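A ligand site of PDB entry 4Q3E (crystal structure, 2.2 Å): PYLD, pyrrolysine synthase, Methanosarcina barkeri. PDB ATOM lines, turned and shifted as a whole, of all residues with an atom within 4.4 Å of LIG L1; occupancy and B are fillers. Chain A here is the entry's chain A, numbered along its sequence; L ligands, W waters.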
ATOM      1  N   PRO A  53     -33.296 -10.384 -22.030  1.00  0.00           N
ATOM      2  CA  PRO A  53     -32.545  -9.550 -21.080  1.00  0.00           C
ATOM      3  C   PRO A  53     -32.504 -10.215 -19.719  1.00  0.00           C
ATOM      4  O   PRO A  53     -33.464 -10.881 -19.329  1.00  0.00           O
ATOM      5  CB  PRO A  53     -33.353  -8.239 -21.018  1.00  0.00           C
ATOM      6  CG  PRO A  53     -34.277  -8.269 -22.185  1.00  0.00           C
ATOM      7  CD  PRO A  53     -34.534  -9.718 -22.481  1.00  0.00           C
ATOM      8  N   VAL A  54     -31.403 -10.022 -18.994  1.00  0.00           N
ATOM      9  CA  VAL A  54     -31.195 -10.649 -17.693  1.00  0.00           C
ATOM     10  C   VAL A  54     -30.758  -9.589 -16.683  1.00  0.00           C
ATOM     11  O   VAL A  54     -29.801  -8.859 -16.928  1.00  0.00           O
ATOM     12  CB  VAL A  54     -30.135 -11.762 -17.787  1.00  0.00           C
ATOM     13  CG1 VAL A  54     -29.725 -12.249 -16.400  1.00  0.00           C
ATOM     14  CG2 VAL A  54     -30.653 -12.912 -18.619  1.00  0.00           C
ATOM     15  N   ILE A  61     -29.309  -3.278 -16.391  1.00  0.00           N
ATOM     16  CA  ILE A  61     -29.489  -3.616 -17.786  1.00  0.00           C
ATOM     17  C   ILE A  61     -29.483  -2.386 -18.671  1.00  0.00           C
ATOM     18  O   ILE A  61     -30.447  -1.614 -18.693  1.00  0.00           O
ATOM     19  CB  ILE A  61     -30.815  -4.359 -18.033  1.00  0.00           C
ATOM     20  CG1 ILE A  61     -30.743  -5.723 -17.348  1.00  0.00           C
ATOM     21  CG2 ILE A  61     -31.075  -4.496 -19.537  1.00  0.00           C
ATOM     22  CD1 ILE A  61     -31.881  -6.642 -17.698  1.00  0.00           C
ATOM     23  N   PHE A  64     -27.339  -4.072 -23.785  1.00  0.00           N
ATOM     24  CA  PHE A  64     -26.735  -5.334 -24.201  1.00  0.00           C
ATOM     25  C   PHE A  64     -27.662  -6.085 -25.144  1.00  0.00           C
ATOM     26  O   PHE A  64     -27.262  -6.452 -26.226  1.00  0.00           O
ATOM     27  CB  PHE A  64     -26.386  -6.231 -23.016  1.00  0.00           C
ATOM     28  CG  PHE A  64     -25.765  -7.555 -23.398  1.00  0.00           C
ATOM     29  CD1 PHE A  64     -24.467  -7.619 -23.888  1.00  0.00           C
ATOM     30  CD2 PHE A  64     -26.485  -8.735 -23.268  1.00  0.00           C
ATOM     31  CE1 PHE A  64     -23.901  -8.820 -24.234  1.00  0.00           C
ATOM     32  CE2 PHE A  64     -25.927  -9.947 -23.609  1.00  0.00           C
ATOM     33  CZ  PHE A  64     -24.633  -9.991 -24.103  1.00  0.00           C
ATOM     34  N   SER A  65     -28.904  -6.283 -24.706  1.00  0.00           N
ATOM     35  CA  SER A  65     -29.928  -6.930 -25.520  1.00  0.00           C
ATOM     36  C   SER A  65     -30.133  -6.169 -26.828  1.00  0.00           C
ATOM     37  O   SER A  65     -30.186  -6.773 -27.894  1.00  0.00           O
ATOM     38  CB  SER A  65     -31.247  -7.029 -24.763  1.00  0.00           C
ATOM     39  OG  SER A  65     -31.105  -7.887 -23.648  1.00  0.00           O
ATOM     40  N   ALA A 104     -27.323 -13.733 -21.301  1.00  0.00           N
ATOM     41  CA  ALA A 104     -26.079 -13.600 -20.546  1.00  0.00           C
ATOM     42  C   ALA A 104     -26.327 -13.042 -19.153  1.00  0.00           C
ATOM     43  O   ALA A 104     -27.099 -12.107 -18.985  1.00  0.00           O
ATOM     44  CB  ALA A 104     -25.124 -12.681 -21.287  1.00  0.00           C
ATOM     45  N   ASP A 105     -25.661 -13.618 -18.150  1.00  0.00           N
ATOM     46  CA  ASP A 105     -25.465 -12.940 -16.877  1.00  0.00           C
ATOM     47  C   ASP A 105     -24.009 -12.435 -16.870  1.00  0.00           C
ATOM     48  O   ASP A 105     -23.348 -12.473 -17.915  1.00  0.00           O
ATOM     49  CB  ASP A 105     -25.839 -13.822 -15.669  1.00  0.00           C
ATOM     50  CG  ASP A 105     -25.017 -15.110 -15.548  1.00  0.00           C
ATOM     51  OD1 ASP A 105     -23.898 -15.195 -16.076  1.00  0.00           O
ATOM     52  OD2 ASP A 105     -25.509 -16.043 -14.884  1.00  0.00           O
ATOM     53  N   ASP A 106     -23.499 -11.950 -15.742  1.00  0.00           N
ATOM     54  CA  ASP A 106     -22.145 -11.384 -15.702  1.00  0.00           C
ATOM     55  C   ASP A 106     -21.040 -12.407 -15.985  1.00  0.00           C
ATOM     56  O   ASP A 106     -19.937 -12.054 -16.405  1.00  0.00           O
ATOM     57  CB  ASP A 106     -21.859 -10.687 -14.373  1.00  0.00           C
ATOM     58  CG  ASP A 106     -20.565  -9.887 -14.402  1.00  0.00           C
ATOM     59  OD1 ASP A 106     -20.355  -9.107 -15.372  1.00  0.00           O
ATOM     60  OD2 ASP A 106     -19.748 -10.033 -13.467  1.00  0.00           O
ATOM     61  N   ASN A 122     -19.815 -17.866 -25.060  1.00  0.00           N
ATOM     62  CA  ASN A 122     -19.156 -16.746 -25.727  1.00  0.00           C
ATOM     63  C   ASN A 122     -17.628 -16.776 -25.657  1.00  0.00           C
ATOM     64  O   ASN A 122     -16.941 -16.413 -26.606  1.00  0.00           O
ATOM     65  CB  ASN A 122     -19.682 -15.437 -25.121  1.00  0.00           C
ATOM     66  CG  ASN A 122     -18.920 -14.213 -25.599  1.00  0.00           C
ATOM     67  OD1 ASN A 122     -18.189 -13.583 -24.845  1.00  0.00           O
ATOM     68  ND2 ASN A 122     -19.123 -13.855 -26.848  1.00  0.00           N
ATOM     69  N   ILE A 227     -10.135  -5.743 -24.576  1.00  0.00           N
ATOM     70  CA  ILE A 227     -10.582  -4.368 -24.389  1.00  0.00           C
ATOM     71  C   ILE A 227      -9.907  -3.820 -23.121  1.00  0.00           C
ATOM     72  O   ILE A 227      -9.981  -4.464 -22.078  1.00  0.00           O
ATOM     73  CB  ILE A 227     -12.124  -4.314 -24.203  1.00  0.00           C
ATOM     74  CG1 ILE A 227     -12.843  -5.024 -25.369  1.00  0.00           C
ATOM     75  CG2 ILE A 227     -12.585  -2.863 -24.129  1.00  0.00           C
ATOM     76  CD1 ILE A 227     -14.287  -5.391 -25.094  1.00  0.00           C
ATOM     77  N   PRO A 247     -16.059  -5.191 -30.598  1.00  0.00           N
ATOM     78  CA  PRO A 247     -16.460  -5.389 -29.196  1.00  0.00           C
ATOM     79  C   PRO A 247     -17.353  -6.584 -28.850  1.00  0.00           C
ATOM     80  O   PRO A 247     -17.355  -7.014 -27.704  1.00  0.00           O
ATOM     81  CB  PRO A 247     -17.189  -4.074 -28.855  1.00  0.00           C
ATOM     82  CG  PRO A 247     -16.862  -3.113 -29.953  1.00  0.00           C
ATOM     83  CD  PRO A 247     -16.609  -3.943 -31.165  1.00  0.00           C
HETATM   84  O1  LIG L   1     -28.843  -8.750 -20.301  1.00  0.00           O
HETATM   85  C1  LIG L   1     -28.089  -7.911 -19.796  1.00  0.00           C
HETATM   86  O2  LIG L   1     -28.334  -6.627 -19.997  1.00  0.00           O
HETATM   87  C2  LIG L   1     -26.894  -8.288 -18.949  1.00  0.00           C
HETATM   88  N1  LIG L   1     -27.196  -9.394 -18.055  1.00  0.00           N
HETATM   89  C3  LIG L   1     -25.763  -8.653 -19.899  1.00  0.00           C
HETATM   90  C4  LIG L   1     -24.423  -8.982 -19.237  1.00  0.00           C
HETATM   91  C5  LIG L   1     -23.440  -9.241 -20.379  1.00  0.00           C
HETATM   92  N2  LIG L   1     -22.135  -9.749 -20.023  1.00  0.00           N
HETATM   93  C6  LIG L   1     -21.123  -8.944 -19.746  1.00  0.00           C
HETATM   94  O3  LIG L   1     -21.256  -7.730 -19.658  1.00  0.00           O
HETATM   95  C7  LIG L   1     -19.753  -9.556 -19.585  1.00  0.00           C
HETATM   96  N3  LIG L   1     -19.207  -9.145 -18.306  1.00  0.00           N
HETATM   97  C8  LIG L   1     -18.814  -9.089 -20.701  1.00  0.00           C
HETATM   98  C9  LIG L   1     -18.993  -9.845 -22.012  1.00  0.00           C
HETATM   99  C10 LIG L   1     -17.767  -9.713 -22.913  1.00  0.00           C
HETATM  100  C11 LIG L   1     -17.668  -8.335 -23.587  1.00  0.00           C
HETATM  101  N4  LIG L   1     -16.390  -7.708 -23.304  1.00  0.00           N
HETATM  102  P1  LG2 L   2      -9.691 -13.658 -18.348  1.00  0.00           P
HETATM  103  O1  LG2 L   2      -9.561 -12.880 -17.083  1.00  0.00           O
HETATM  104  O2  LG2 L   2     -10.187 -15.070 -18.326  1.00  0.00           O
HETATM  105  O3  LG2 L   2      -8.276 -13.727 -19.097  1.00  0.00           O
HETATM  106  C1  LG2 L   2      -7.483 -12.568 -19.242  1.00  0.00           C
HETATM  107  C2  LG2 L   2      -6.042 -12.995 -19.057  1.00  0.00           C
HETATM  108  O4  LG2 L   2      -5.170 -11.951 -19.453  1.00  0.00           O
HETATM  109  C3  LG2 L   2      -5.695 -13.323 -17.611  1.00  0.00           C
HETATM  110  O5  LG2 L   2      -5.347 -14.706 -17.519  1.00  0.00           O
HETATM  111  C4  LG2 L   2      -4.513 -12.429 -17.267  1.00  0.00           C
HETATM  112  O6  LG2 L   2      -3.522 -13.072 -16.459  1.00  0.00           O
HETATM  113  C5  LG2 L   2      -4.009 -12.074 -18.656  1.00  0.00           C
HETATM  114  N1  LG2 L   2      -3.220 -10.834 -18.716  1.00  0.00           N
HETATM  115  C6  LG2 L   2      -3.497  -9.651 -18.136  1.00  0.00           C
HETATM  116  N2  LG2 L   2      -2.518  -8.748 -18.415  1.00  0.00           N
HETATM  117  C7  LG2 L   2      -1.607  -9.365 -19.187  1.00  0.00           C
HETATM  118  C8  LG2 L   2      -0.336  -9.012 -19.839  1.00  0.00           C
HETATM  119  N3  LG2 L   2       0.155  -7.764 -19.706  1.00  0.00           N
HETATM  120  N4  LG2 L   2       0.307  -9.953 -20.572  1.00  0.00           N
HETATM  121  C9  LG2 L   2      -0.184 -11.200 -20.706  1.00  0.00           C
HETATM  122  N5  LG2 L   2      -1.339 -11.591 -20.131  1.00  0.00           N
HETATM  123  C10 LG2 L   2      -2.072 -10.736 -19.380  1.00  0.00           C
HETATM  124  O7  LG2 L   2     -10.541 -12.769 -19.385  1.00  0.00           O
HETATM  125  P2  LG2 L   2     -11.241 -13.405 -20.696  1.00  0.00           P
HETATM  126  O8  LG2 L   2     -12.577 -13.940 -20.244  1.00  0.00           O
HETATM  127  O9  LG2 L   2     -10.257 -14.308 -21.409  1.00  0.00           O
HETATM  128  O10 LG2 L   2     -11.484 -12.052 -21.522  1.00  0.00           O
HETATM  129  C11 LG2 L   2     -10.408 -11.403 -22.179  1.00  0.00           C
HETATM  130  C12 LG2 L   2     -10.844 -10.043 -22.713  1.00  0.00           C
HETATM  131  O11 LG2 L   2     -11.698 -10.207 -23.842  1.00  0.00           O
HETATM  132  C13 LG2 L   2     -11.640  -9.179 -21.730  1.00  0.00           C
HETATM  133  O12 LG2 L   2     -11.282  -7.821 -21.967  1.00  0.00           O
HETATM  134  C14 LG2 L   2     -13.090  -9.387 -22.134  1.00  0.00           C
HETATM  135  O13 LG2 L   2     -13.890  -8.275 -21.759  1.00  0.00           O
HETATM  136  C15 LG2 L   2     -12.930  -9.497 -23.639  1.00  0.00           C
HETATM  137  N6  LG2 L   2     -13.958 -10.177 -24.411  1.00  0.00           N
HETATM  138  C16 LG2 L   2     -14.249  -9.637 -25.609  1.00  0.00           C
HETATM  139  C17 LG2 L   2     -15.183 -10.183 -26.468  1.00  0.00           C
HETATM  140  C18 LG2 L   2     -15.450  -9.535 -27.812  1.00  0.00           C
HETATM  141  O14 LG2 L   2     -16.367  -9.948 -28.508  1.00  0.00           O
HETATM  142  N7  LG2 L   2     -14.662  -8.551 -28.263  1.00  0.00           N
HETATM  143  C19 LG2 L   2     -15.915 -11.441 -26.075  1.00  0.00           C
HETATM  144  C20 LG2 L   2     -15.497 -11.955 -24.770  1.00  0.00           C
HETATM  145  C21 LG2 L   2     -14.540 -11.309 -24.000  1.00  0.00           C
HETATM  146  O   HOH W   1     -17.697 -13.088 -22.269  1.00  0.00           O
HETATM  147  O   HOH W   2     -29.049 -11.417 -21.791  1.00  0.00           O
HETATM  148  O   HOH W   3     -25.653  -9.592 -15.645  1.00  0.00           O
HETATM  149  O   HOH W   4     -26.916  -4.468 -20.530  1.00  0.00           O
HETATM  150  O   HOH W   5     -21.471 -12.655 -19.921  1.00  0.00           O
HETATM  151  O   HOH W   6     -29.974  -6.164 -21.893  1.00  0.00           O
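A nitrogen (N4) of LIG L1 is in hydrogen-bond range of an oxygen (O13) of LG2 L2, at 3.0 Å.
Water W6 lies within hydrogen-bond range of O2 of LIG L1 (2.5 Å) and OG of Ser 65 (2.7 Å).
Water W4 lies within hydrogen-bond range of O2 of LIG L1 and N of Phe 64.
Water W3 lies within hydrogen-bond range of N1 of LIG L1 (2.9 Å) and N of Asp 106 (3.2 Å).
Water W5 lies within hydrogen-bond range of O of Asp 105 (2.8 Å) and N2 of LIG L1 (3.0 Å).
Water W2 lies within hydrogen-bond range of N of Ala 104 and O1 of LIG L1.
CA of Pro 53 touches O1 of LIG L1, at 3.9 Å.
CG2 of Ile 61 touches O2 of LIG L1, 3.5 Å away.
CD2 of Phe 64 touches C3 of LIG L1, 3.4 Å away.
Asp 105 touches LIG L1.
Ile 227 touches LIG L1.
Of the 11 residues printed, 8 come within 4 Å of LIG L1.
N1 of LIG L1 sits at hydrogen-bond distance from O of Ala 104.
An oxygen (O1) of LIG L1 lies within hydrogen-bond range of the backbone NH of Val 54 (3.1 Å).
N1 of LIG L1 lies within hydrogen-bond range of O of Val 54, 2.9 Å away.
A nitrogen (N3) of LIG L1 is in salt-bridge range of the side-chain carboxylate (OD1) of Asp 106, 3.2 Å away.
The backbone carbonyl oxygen (O) of Pro 247 sits at hydrogen-bond distance from a nitrogen (N7) of LG2 L2 (3.2 Å).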
